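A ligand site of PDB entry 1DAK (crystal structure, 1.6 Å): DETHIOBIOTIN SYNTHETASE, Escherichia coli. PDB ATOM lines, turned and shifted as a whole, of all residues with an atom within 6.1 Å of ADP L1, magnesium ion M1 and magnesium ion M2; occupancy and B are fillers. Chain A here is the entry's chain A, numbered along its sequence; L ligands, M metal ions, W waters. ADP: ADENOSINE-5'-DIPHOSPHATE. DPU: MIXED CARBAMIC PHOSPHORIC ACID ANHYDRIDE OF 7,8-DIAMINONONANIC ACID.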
ATOM      1  N   GLY A   8     -12.508 -21.165  -2.819  1.00  0.00           N
ATOM      2  CA  GLY A   8     -12.213 -19.903  -2.163  1.00  0.00           C
ATOM      3  C   GLY A   8     -10.721 -19.779  -1.870  1.00  0.00           C
ATOM      4  O   GLY A   8      -9.960 -20.734  -1.877  1.00  0.00           O
ATOM      5  N   ASP A  10      -9.584 -19.268   0.957  1.00  0.00           N
ATOM      6  CA  ASP A  10      -9.415 -19.944   2.241  1.00  0.00           C
ATOM      7  C   ASP A  10     -10.786 -20.439   2.692  1.00  0.00           C
ATOM      8  O   ASP A  10     -11.775 -20.279   1.964  1.00  0.00           O
ATOM      9  CB  ASP A  10      -8.829 -18.948   3.244  1.00  0.00           C
ATOM     10  CG  ASP A  10      -8.303 -19.536   4.535  1.00  0.00           C
ATOM     11  OD1 ASP A  10      -8.345 -20.765   4.715  1.00  0.00           O
ATOM     12  OD2 ASP A  10      -7.842 -18.754   5.389  1.00  0.00           O
ATOM     13  N   THR A  11     -10.859 -21.008   3.891  1.00  0.00           N
ATOM     14  CA  THR A  11     -12.170 -21.268   4.496  1.00  0.00           C
ATOM     15  C   THR A  11     -12.558 -19.917   5.107  1.00  0.00           C
ATOM     16  O   THR A  11     -11.727 -19.040   5.289  1.00  0.00           O
ATOM     17  CB  THR A  11     -12.143 -22.377   5.552  1.00  0.00           C
ATOM     18  OG1 THR A  11     -13.474 -22.688   6.003  1.00  0.00           O
ATOM     19  CG2 THR A  11     -11.315 -21.967   6.757  1.00  0.00           C
ATOM     20  N   GLU A  12     -13.820 -19.659   5.355  1.00  0.00           N
ATOM     21  CA  GLU A  12     -14.347 -18.438   5.951  1.00  0.00           C
ATOM     22  C   GLU A  12     -14.110 -17.169   5.151  1.00  0.00           C
ATOM     23  O   GLU A  12     -13.816 -16.135   5.738  1.00  0.00           O
ATOM     24  CB  GLU A  12     -13.816 -18.288   7.387  1.00  0.00           C
ATOM     25  CG  GLU A  12     -14.721 -17.447   8.272  1.00  0.00           C
ATOM     26  CD  GLU A  12     -15.910 -18.192   8.837  1.00  0.00           C
ATOM     27  OE1 GLU A  12     -15.930 -19.439   8.818  1.00  0.00           O
ATOM     28  OE2 GLU A  12     -16.841 -17.527   9.346  1.00  0.00           O
ATOM     29  N   VAL A  13     -14.245 -17.199   3.834  1.00  0.00           N
ATOM     30  CA  VAL A  13     -14.052 -16.064   2.957  1.00  0.00           C
ATOM     31  C   VAL A  13     -15.295 -15.650   2.175  1.00  0.00           C
ATOM     32  O   VAL A  13     -15.305 -14.597   1.534  1.00  0.00           O
ATOM     33  CB  VAL A  13     -12.923 -16.287   1.933  1.00  0.00           C
ATOM     34  CG1 VAL A  13     -11.590 -16.505   2.638  1.00  0.00           C
ATOM     35  CG2 VAL A  13     -13.197 -17.425   0.970  1.00  0.00           C
ATOM     36  N   GLY A  14     -16.322 -16.475   2.177  1.00  0.00           N
ATOM     37  CA  GLY A  14     -17.548 -16.179   1.449  1.00  0.00           C
ATOM     38  C   GLY A  14     -17.973 -17.145   0.375  1.00  0.00           C
ATOM     39  O   GLY A  14     -18.859 -16.825  -0.432  1.00  0.00           O
ATOM     40  N   LYS A  15     -17.440 -18.356   0.301  1.00  0.00           N
ATOM     41  CA  LYS A  15     -17.856 -19.308  -0.727  1.00  0.00           C
ATOM     42  C   LYS A  15     -19.373 -19.489  -0.662  1.00  0.00           C
ATOM     43  O   LYS A  15     -20.015 -19.484  -1.694  1.00  0.00           O
ATOM     44  CB  LYS A  15     -17.211 -20.697  -0.647  1.00  0.00           C
ATOM     45  CG  LYS A  15     -15.713 -20.734  -0.879  1.00  0.00           C
ATOM     46  CD  LYS A  15     -15.187 -22.170  -0.869  1.00  0.00           C
ATOM     47  CE  LYS A  15     -15.408 -22.880   0.451  1.00  0.00           C
ATOM     48  NZ  LYS A  15     -14.530 -22.329   1.525  1.00  0.00           N
ATOM     49  N   THR A  16     -19.934 -19.677   0.524  1.00  0.00           N
ATOM     50  CA  THR A  16     -21.351 -19.994   0.681  1.00  0.00           C
ATOM     51  C   THR A  16     -22.183 -18.766   0.335  1.00  0.00           C
ATOM     52  O   THR A  16     -23.098 -18.900  -0.478  1.00  0.00           O
ATOM     53  CB  THR A  16     -21.689 -20.554   2.065  1.00  0.00           C
ATOM     54  OG1 THR A  16     -20.935 -21.769   2.257  1.00  0.00           O
ATOM     55  CG2 THR A  16     -23.162 -20.849   2.256  1.00  0.00           C
ATOM     56  N   VAL A  17     -21.805 -17.593   0.832  1.00  0.00           N
ATOM     57  CA  VAL A  17     -22.580 -16.389   0.465  1.00  0.00           C
ATOM     58  C   VAL A  17     -22.531 -16.148  -1.033  1.00  0.00           C
ATOM     59  O   VAL A  17     -23.562 -15.876  -1.679  1.00  0.00           O
ATOM     60  CB  VAL A  17     -22.047 -15.185   1.252  1.00  0.00           C
ATOM     61  CG1 VAL A  17     -22.549 -13.861   0.676  1.00  0.00           C
ATOM     62  CG2 VAL A  17     -22.488 -15.325   2.705  1.00  0.00           C
ATOM     63  N   ALA A  18     -21.357 -16.242  -1.649  1.00  0.00           N
ATOM     64  CA  ALA A  18     -21.207 -16.063  -3.091  1.00  0.00           C
ATOM     65  C   ALA A  18     -21.947 -17.138  -3.874  1.00  0.00           C
ATOM     66  O   ALA A  18     -22.532 -16.850  -4.921  1.00  0.00           O
ATOM     67  CB  ALA A  18     -19.736 -16.037  -3.490  1.00  0.00           C
ATOM     68  N   LYS A  37     -23.188 -29.594  -2.017  1.00  0.00           N
ATOM     69  CA  LYS A  37     -22.052 -29.495  -1.067  1.00  0.00           C
ATOM     70  C   LYS A  37     -21.757 -30.946  -0.698  1.00  0.00           C
ATOM     71  O   LYS A  37     -22.300 -31.435   0.296  1.00  0.00           O
ATOM     72  CB  LYS A  37     -22.473 -28.691   0.154  1.00  0.00           C
ATOM     73  CG  LYS A  37     -21.469 -28.613   1.306  1.00  0.00           C
ATOM     74  CD  LYS A  37     -20.504 -27.448   1.190  1.00  0.00           C
ATOM     75  CE  LYS A  37     -19.559 -27.416   2.385  1.00  0.00           C
ATOM     76  NZ  LYS A  37     -18.613 -26.250   2.319  1.00  0.00           N
ATOM     77  N   ASP A  54     -24.004 -24.630   5.519  1.00  0.00           N
ATOM     78  CA  ASP A  54     -23.700 -24.328   4.126  1.00  0.00           C
ATOM     79  C   ASP A  54     -24.674 -25.083   3.230  1.00  0.00           C
ATOM     80  O   ASP A  54     -25.291 -24.535   2.317  1.00  0.00           O
ATOM     81  CB  ASP A  54     -22.291 -24.757   3.693  1.00  0.00           C
ATOM     82  CG  ASP A  54     -21.149 -23.959   4.260  1.00  0.00           C
ATOM     83  OD1 ASP A  54     -21.352 -23.169   5.204  1.00  0.00           O
ATOM     84  OD2 ASP A  54     -20.037 -24.098   3.709  1.00  0.00           O
ATOM     85  N   GLU A 115     -20.220 -26.500  -4.166  1.00  0.00           N
ATOM     86  CA  GLU A 115     -19.361 -25.746  -3.251  1.00  0.00           C
ATOM     87  C   GLU A 115     -18.353 -26.714  -2.633  1.00  0.00           C
ATOM     88  O   GLU A 115     -18.756 -27.772  -2.152  1.00  0.00           O
ATOM     89  CB  GLU A 115     -20.122 -25.019  -2.143  1.00  0.00           C
ATOM     90  CG  GLU A 115     -19.209 -24.161  -1.267  1.00  0.00           C
ATOM     91  CD  GLU A 115     -19.746 -23.636   0.038  1.00  0.00           C
ATOM     92  OE1 GLU A 115     -20.974 -23.516   0.213  1.00  0.00           O
ATOM     93  OE2 GLU A 115     -18.949 -23.291   0.957  1.00  0.00           O
ATOM     94  N   GLY A 116     -17.086 -26.327  -2.690  1.00  0.00           N
ATOM     95  CA  GLY A 116     -16.040 -27.161  -2.061  1.00  0.00           C
ATOM     96  C   GLY A 116     -16.057 -26.939  -0.547  1.00  0.00           C
ATOM     97  O   GLY A 116     -16.991 -26.399   0.022  1.00  0.00           O
ATOM     98  N   GLY A 118     -13.392 -25.670   2.565  1.00  0.00           N
ATOM     99  CA  GLY A 118     -12.109 -24.989   2.770  1.00  0.00           C
ATOM    100  C   GLY A 118     -11.623 -24.437   1.438  1.00  0.00           C
ATOM    101  O   GLY A 118     -12.416 -23.919   0.625  1.00  0.00           O
ATOM    102  N   ASN A 175     -15.707 -10.780  -2.604  1.00  0.00           N
ATOM    103  CA  ASN A 175     -16.631 -10.769  -1.472  1.00  0.00           C
ATOM    104  C   ASN A 175     -16.110  -9.853  -0.376  1.00  0.00           C
ATOM    105  O   ASN A 175     -15.004 -10.020   0.144  1.00  0.00           O
ATOM    106  CB  ASN A 175     -16.855 -12.198  -0.951  1.00  0.00           C
ATOM    107  CG  ASN A 175     -17.923 -12.220   0.128  1.00  0.00           C
ATOM    108  OD1 ASN A 175     -19.018 -11.665  -0.045  1.00  0.00           O
ATOM    109  ND2 ASN A 175     -17.677 -12.826   1.280  1.00  0.00           N
ATOM    110  N   ASP A 176     -16.889  -8.823  -0.049  1.00  0.00           N
ATOM    111  CA  ASP A 176     -16.528  -7.846   0.964  1.00  0.00           C
ATOM    112  C   ASP A 176     -16.882  -8.381   2.339  1.00  0.00           C
ATOM    113  O   ASP A 176     -17.964  -8.148   2.894  1.00  0.00           O
ATOM    114  CB  ASP A 176     -17.234  -6.523   0.655  1.00  0.00           C
ATOM    115  CG  ASP A 176     -16.868  -5.972  -0.710  1.00  0.00           C
ATOM    116  OD1 ASP A 176     -15.929  -6.472  -1.358  1.00  0.00           O
ATOM    117  OD2 ASP A 176     -17.528  -5.010  -1.182  1.00  0.00           O
ATOM    118  N   VAL A 177     -15.946  -9.114   2.951  1.00  0.00           N
ATOM    119  CA  VAL A 177     -16.137  -9.740   4.244  1.00  0.00           C
ATOM    120  C   VAL A 177     -16.198  -8.733   5.379  1.00  0.00           C
ATOM    121  O   VAL A 177     -16.731  -9.026   6.449  1.00  0.00           O
ATOM    122  CB  VAL A 177     -15.062 -10.812   4.520  1.00  0.00           C
ATOM    123  CG1 VAL A 177     -15.335 -12.038   3.661  1.00  0.00           C
ATOM    124  CG2 VAL A 177     -13.658 -10.291   4.255  1.00  0.00           C
ATOM    125  N   THR A 178     -15.631  -7.540   5.202  1.00  0.00           N
ATOM    126  CA  THR A 178     -15.663  -6.500   6.213  1.00  0.00           C
ATOM    127  C   THR A 178     -16.069  -5.176   5.562  1.00  0.00           C
ATOM    128  O   THR A 178     -16.029  -5.070   4.347  1.00  0.00           O
ATOM    129  CB  THR A 178     -14.294  -6.250   6.883  1.00  0.00           C
ATOM    130  OG1 THR A 178     -13.350  -5.835   5.889  1.00  0.00           O
ATOM    131  CG2 THR A 178     -13.779  -7.479   7.601  1.00  0.00           C
ATOM    132  N   ILE A 203     -19.848  -8.748  -4.037  1.00  0.00           N
ATOM    133  CA  ILE A 203     -20.892  -8.796  -3.007  1.00  0.00           C
ATOM    134  C   ILE A 203     -20.502  -7.861  -1.873  1.00  0.00           C
ATOM    135  O   ILE A 203     -19.408  -7.982  -1.321  1.00  0.00           O
ATOM    136  CB  ILE A 203     -21.083 -10.221  -2.471  1.00  0.00           C
ATOM    137  CG1 ILE A 203     -21.394 -11.136  -3.662  1.00  0.00           C
ATOM    138  CG2 ILE A 203     -22.180 -10.268  -1.418  1.00  0.00           C
ATOM    139  CD1 ILE A 203     -21.325 -12.608  -3.355  1.00  0.00           C
ATOM    140  N   PRO A 204     -21.338  -6.881  -1.598  1.00  0.00           N
ATOM    141  CA  PRO A 204     -21.037  -5.910  -0.562  1.00  0.00           C
ATOM    142  C   PRO A 204     -21.087  -6.507   0.833  1.00  0.00           C
ATOM    143  O   PRO A 204     -21.602  -7.607   1.050  1.00  0.00           O
ATOM    144  CB  PRO A 204     -22.097  -4.822  -0.741  1.00  0.00           C
ATOM    145  CG  PRO A 204     -23.201  -5.436  -1.503  1.00  0.00           C
ATOM    146  CD  PRO A 204     -22.670  -6.643  -2.226  1.00  0.00           C
ATOM    147  N   TRP A 205     -20.549  -5.743   1.782  1.00  0.00           N
ATOM    148  CA  TRP A 205     -20.588  -6.171   3.184  1.00  0.00           C
ATOM    149  C   TRP A 205     -22.018  -6.100   3.688  1.00  0.00           C
ATOM    150  O   TRP A 205     -22.624  -5.030   3.786  1.00  0.00           O
ATOM    151  CB  TRP A 205     -19.644  -5.301   4.032  1.00  0.00           C
ATOM    152  CG  TRP A 205     -19.736  -5.629   5.492  1.00  0.00           C
ATOM    153  CD1 TRP A 205     -19.303  -6.777   6.092  1.00  0.00           C
ATOM    154  CD2 TRP A 205     -20.272  -4.806   6.526  1.00  0.00           C
ATOM    155  NE1 TRP A 205     -19.553  -6.721   7.442  1.00  0.00           N
ATOM    156  CE2 TRP A 205     -20.149  -5.527   7.738  1.00  0.00           C
ATOM    157  CE3 TRP A 205     -20.858  -3.533   6.557  1.00  0.00           C
ATOM    158  CZ2 TRP A 205     -20.585  -5.022   8.956  1.00  0.00           C
ATOM    159  CZ3 TRP A 205     -21.286  -3.040   7.772  1.00  0.00           C
ATOM    160  CH2 TRP A 205     -21.151  -3.773   8.959  1.00  0.00           C
ATOM    161  N   LEU A 206     -22.594  -7.264   3.980  1.00  0.00           N
ATOM    162  CA  LEU A 206     -23.959  -7.379   4.450  1.00  0.00           C
ATOM    163  C   LEU A 206     -23.963  -8.053   5.821  1.00  0.00           C
ATOM    164  O   LEU A 206     -23.967  -9.287   5.912  1.00  0.00           O
ATOM    165  CB  LEU A 206     -24.782  -8.185   3.445  1.00  0.00           C
ATOM    166  CG  LEU A 206     -24.990  -7.528   2.078  1.00  0.00           C
ATOM    167  CD1 LEU A 206     -25.336  -8.552   1.010  1.00  0.00           C
ATOM    168  CD2 LEU A 206     -26.075  -6.467   2.168  1.00  0.00           C
ATOM    169  N   ALA A 207     -23.873  -7.254   6.865  1.00  0.00           N
ATOM    170  CA  ALA A 207     -23.804  -7.755   8.233  1.00  0.00           C
ATOM    171  C   ALA A 207     -24.831  -8.810   8.606  1.00  0.00           C
ATOM    172  O   ALA A 207     -24.448  -9.875   9.116  1.00  0.00           O
ATOM    173  CB  ALA A 207     -23.899  -6.569   9.189  1.00  0.00           C
ATOM    174  N   ASN A 209     -27.418 -11.767   8.154  1.00  0.00           N
ATOM    175  CA  ASN A 209     -27.740 -12.938   7.366  1.00  0.00           C
ATOM    176  C   ASN A 209     -27.604 -12.746   5.862  1.00  0.00           C
ATOM    177  O   ASN A 209     -28.565 -12.756   5.099  1.00  0.00           O
ATOM    178  CB  ASN A 209     -29.160 -13.415   7.699  1.00  0.00           C
ATOM    179  CG  ASN A 209     -29.335 -13.670   9.191  1.00  0.00           C
ATOM    180  OD1 ASN A 209     -29.333 -12.729  10.000  1.00  0.00           O
ATOM    181  ND2 ASN A 209     -29.502 -14.932   9.571  1.00  0.00           N
ATOM    182  N   PRO A 210     -26.352 -12.716   5.392  1.00  0.00           N
ATOM    183  CA  PRO A 210     -26.045 -12.536   3.989  1.00  0.00           C
ATOM    184  C   PRO A 210     -26.431 -13.703   3.095  1.00  0.00           C
ATOM    185  O   PRO A 210     -26.641 -13.547   1.892  1.00  0.00           O
ATOM    186  CB  PRO A 210     -24.541 -12.274   3.963  1.00  0.00           C
ATOM    187  CG  PRO A 210     -24.023 -12.895   5.218  1.00  0.00           C
ATOM    188  CD  PRO A 210     -25.122 -12.746   6.233  1.00  0.00           C
ATOM    189  N   GLU A 211     -26.562 -14.895   3.677  1.00  0.00           N
ATOM    190  CA  GLU A 211     -26.949 -16.105   2.963  1.00  0.00           C
ATOM    191  C   GLU A 211     -28.376 -16.042   2.425  1.00  0.00           C
ATOM    192  O   GLU A 211     -28.706 -16.673   1.424  1.00  0.00           O
ATOM    193  CB  GLU A 211     -26.784 -17.329   3.874  1.00  0.00           C
ATOM    194  CG  GLU A 211     -25.392 -17.656   4.344  1.00  0.00           C
ATOM    195  CD  GLU A 211     -24.879 -16.844   5.514  1.00  0.00           C
ATOM    196  OE1 GLU A 211     -25.659 -16.078   6.118  1.00  0.00           O
ATOM    197  OE2 GLU A 211     -23.682 -16.937   5.858  1.00  0.00           O
HETATM  198  PB  ADP L   1     -16.819 -19.918   3.367  1.00  0.00           P
HETATM  199  O1B ADP L   1     -15.666 -19.657   2.514  1.00  0.00           O
HETATM  200  O2B ADP L   1     -16.603 -20.656   4.644  1.00  0.00           O
HETATM  201  O3B ADP L   1     -18.113 -20.620   2.753  1.00  0.00           O
HETATM  202  PA  ADP L   1     -19.138 -18.084   4.180  1.00  0.00           P
HETATM  203  O1A ADP L   1     -19.750 -19.126   5.076  1.00  0.00           O
HETATM  204  O2A ADP L   1     -19.930 -17.726   2.973  1.00  0.00           O
HETATM  205  O3A ADP L   1     -17.521 -18.480   3.782  1.00  0.00           O
HETATM  206  O5' ADP L   1     -18.801 -16.688   5.020  1.00  0.00           O
HETATM  207  C5' ADP L   1     -17.923 -16.804   6.209  1.00  0.00           C
HETATM  208  C4' ADP L   1     -18.528 -15.931   7.307  1.00  0.00           C
HETATM  209  O4' ADP L   1     -18.509 -14.575   6.857  1.00  0.00           O
HETATM  210  C3' ADP L   1     -20.003 -16.253   7.572  1.00  0.00           C
HETATM  211  O3' ADP L   1     -20.370 -16.042   8.958  1.00  0.00           O
HETATM  212  C2' ADP L   1     -20.786 -15.308   6.660  1.00  0.00           C
HETATM  213  O2' ADP L   1     -22.119 -15.063   7.161  1.00  0.00           O
HETATM  214  C1' ADP L   1     -19.880 -14.067   6.684  1.00  0.00           C
HETATM  215  N9  ADP L   1     -20.015 -13.329   5.360  1.00  0.00           N
HETATM  216  C8  ADP L   1     -19.635 -13.832   4.188  1.00  0.00           C
HETATM  217  N7  ADP L   1     -19.728 -12.892   3.259  1.00  0.00           N
HETATM  218  C5  ADP L   1     -20.302 -11.816   3.783  1.00  0.00           C
HETATM  219  C6  ADP L   1     -20.625 -10.573   3.249  1.00  0.00           C
HETATM  220  N6  ADP L   1     -20.409 -10.255   1.964  1.00  0.00           N
HETATM  221  N1  ADP L   1     -20.924  -9.610   4.145  1.00  0.00           N
HETATM  222  C2  ADP L   1     -20.901  -9.836   5.463  1.00  0.00           C
HETATM  223  N3  ADP L   1     -20.795 -11.069   5.984  1.00  0.00           N
HETATM  224  C4  ADP L   1     -20.367 -12.047   5.146  1.00  0.00           C
HETATM  225  CA  DPU L   2      -8.338 -27.737   5.454  1.00  0.00           C
HETATM  226  C   DPU L   2      -6.996 -26.963   5.532  1.00  0.00           C
HETATM  227  OI1 DPU L   2      -6.475 -26.785   6.657  1.00  0.00           O
HETATM  228  OI2 DPU L   2      -6.616 -26.443   4.457  1.00  0.00           O
HETATM  229  CB  DPU L   2      -9.415 -26.823   6.085  1.00  0.00           C
HETATM  230  CG  DPU L   2     -10.816 -27.424   5.965  1.00  0.00           C
HETATM  231  CD  DPU L   2     -11.981 -26.495   6.399  1.00  0.00           C
HETATM  232  CE  DPU L   2     -13.347 -27.236   6.220  1.00  0.00           C
HETATM  233  CZ  DPU L   2     -14.537 -26.393   6.551  1.00  0.00           C
HETATM  234  CH  DPU L   2     -14.594 -25.437   7.762  1.00  0.00           C
HETATM  235  CS  DPU L   2     -14.674 -26.284   9.049  1.00  0.00           C
HETATM  236  N1  DPU L   2     -15.859 -27.443   6.328  1.00  0.00           N
HETATM  237  N2  DPU L   2     -15.932 -24.717   7.682  1.00  0.00           N
HETATM  238  CN1 DPU L   2     -16.797 -26.995   5.383  1.00  0.00           C
HETATM  239  O12 DPU L   2     -17.767 -27.825   5.245  1.00  0.00           O
HETATM  240  O2B DPU L   2     -17.075 -23.653   3.151  1.00  0.00           O
HETATM  241  PB  DPU L   2     -16.140 -24.057   4.170  1.00  0.00           P
HETATM  242  O1B DPU L   2     -16.444 -25.862   4.110  1.00  0.00           O
HETATM  243  O3B DPU L   2     -16.677 -23.672   5.496  1.00  0.00           O
HETATM  244  O2A DPU L   2     -14.698 -23.584   3.886  1.00  0.00           O
HETATM  245 MG    MG M   1     -18.903 -22.463   2.940  1.00  0.00          MG
HETATM  246 MG    MG M   2     -17.422 -21.826   6.186  1.00  0.00          MG
HETATM  247  O   HOH W   1     -15.645 -21.600   7.552  1.00  0.00           O
HETATM  248  O   HOH W   2     -18.267 -22.869   7.798  1.00  0.00           O
HETATM  249  O   HOH W   3     -19.025 -17.750  10.364  1.00  0.00           O
HETATM  250  O   HOH W   4     -22.311 -13.383   9.784  1.00  0.00           O
HETATM  251  O   HOH W   5     -18.148 -20.112   7.317  1.00  0.00           O
HETATM  252  O   HOH W   6     -22.191 -19.035   6.117  1.00  0.00           O
HETATM  253  O   HOH W   7     -21.471 -11.140   8.702  1.00  0.00           O
HETATM  254  O   HOH W   8     -19.160 -21.738   5.071  1.00  0.00           O
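Lys 37 touches magnesium ion M1. Within 4 Å of magnesium ion M1: Thr 16, Lys 37, Asp 54 and Glu 115.
The backbone NH of Thr 16 lies within hydrogen-bond range of an oxygen (O2A) of ADP L1 (3.1 Å). The side-chain carboxylate of Glu 211 is in hydrogen-bond range of an oxygen (O2') of ADP L1, 2.8 Å away. The side-chain amide oxygen (OD1) of Asn 175 is in hydrogen-bond range of a nitrogen (N6) of ADP L1. An oxygen (O3A) of ADP L1 sits at hydrogen-bond distance from the backbone NH (N) of Gly 14 (2.8 Å). The backbone NH of Val 17 lies within hydrogen-bond range of an oxygen (O2A) of ADP L1 (2.8 Å). N of Leu 206 lies within hydrogen-bond range of N1 of ADP L1 (2.9 Å). The backbone NH (N) of Glu 12 is in hydrogen-bond range of an oxygen (O1B) of ADP L1, at 3.4 Å. A nitrogen (N6) of ADP L1 is in hydrogen-bond range of the backbone carbonyl oxygen (O) of Pro 204, at 3.0 Å. An oxygen (O1B) of ADP L1 lies within hydrogen-bond range of the backbone NH (N) of Lys 15 (3.1 Å). NZ of Lys 15 is in salt-bridge range of O1B of ADP L1 (3.1 Å). The backbone NH (N) of Val 13 lies within hydrogen-bond range of an oxygen (O1B) of ADP L1, at 3.1 Å. The backbone carbonyl oxygen (O) of Asp 176 lies within hydrogen-bond range of a nitrogen (N6) of ADP L1 (3.4 Å). An oxygen (O2A) of DPU L2 is in salt-bridge range of the side-chain amino group of Lys 15, 2.7 Å away. An oxygen (O1B) of DPU L2 sits at hydrogen-bond distance from the side-chain amino group of Lys 37, 2.8 Å away. O2A of DPU L2 lies within hydrogen-bond range of OG1 of Thr 11. N of Gly 118 is in hydrogen-bond range of O2A of DPU L2 (2.8 Å).
An oxygen (O3B) of ADP L1 is bound to magnesium ion M1. OD2 of Asp 54 binds magnesium ion M1 (2.1 Å). OE2 of Glu 115 binds magnesium ion M1 (2.1 Å). O2B of DPU L2 is bound to magnesium ion M1, 2.2 Å away. Magnesium ion M1 is bound by OG1 of Thr 16 (2.3 Å). Water W8 binds magnesium ion M1 (2.3 Å). Magnesium ion M1 has six donor atoms within binding distance.
Asp 10 touches ADP L1 (O to O1B, 3.98 Å). Thr 11 touches ADP L1. Ile 203 touches ADP L1 (CG2 to N6, 3.8 Å). CD1 of Trp 205 touches C2 of ADP L1, 3.5 Å away. CG of Pro 210 touches O2' of ADP L1 (3.5 Å). Of the 27 residues printed, 17 come within 4 Å of ADP L1. The nearest printed residue that does not touch ADP L1 is Asp 54 (4.1 Å).
Residues that only touch magnesium ion M2: Glu 12 (3.9 Å). Of the 27 residues printed, 1 comes within 4 Å of magnesium ion M2. The nearest printed residue that does not touch magnesium ion M2 is Thr 11 (4.05 Å).
Water W8 bridges the side-chain carboxylate of Asp 54 (2.6 Å) and an oxygen (O1A) of ADP L1 (2.7 Å). Water W1 lies within hydrogen-bond range of the side-chain carboxylate (OE1) of Glu 12, the side-chain hydroxyl (OG1) of Thr 11 and a nitrogen (N2) of DPU L2. Water W5 bridges the side-chain carboxylate (OE1) of Glu 12 (2.8 Å) and an oxygen (O1A) of ADP L1 (2.9 Å). Water W3 lies within hydrogen-bond range of the side-chain carboxylate (OE2) of Glu 12 (2.4 Å) and an oxygen (O3') of ADP L1 (2.6 Å). Water W6 lies within hydrogen-bond range of OE2 of Glu 211 and O1A of ADP L1. Water W7 bridges N3 of ADP L1 (2.8 Å) and O of Ala 207 (3.3 Å).
Magnesium ion M2 is bound by water W8 (2.1 Å), water W2 (2.1 Å), O2B of ADP L1 (2.1 Å), O3B of DPU L2 (2.1 Å), water W5 (2.2 Å) and water W1 (2.3 Å). Magnesium ion M2 has six donor atoms within binding distance.
The side-chain amino group (NZ) of Lys 37 sits close to the side-chain carboxylate (OD2) of Asp 54 (2.9 Å). The side-chain carboxylate of Glu 115 lies close to the side-chain amino group of Lys 37, at 3.3 Å. ND2 of Asn 175 lies within hydrogen-bond range of O of Val 13 (3.0 Å). The backbone carbonyl oxygen of Asp 10 sits at hydrogen-bond distance from the side-chain amino group of Lys 15 (3.5 Å). O of Gly 118 lies within hydrogen-bond range of NZ of Lys 15, at 2.8 Å. The backbone carbonyl oxygen (O) of Ile 203 lies within hydrogen-bond range of the backbone NH (N) of Asp 176 (2.9 Å). NZ of Lys 37 lies within hydrogen-bond range of O of Gly 116, 2.8 Å away.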
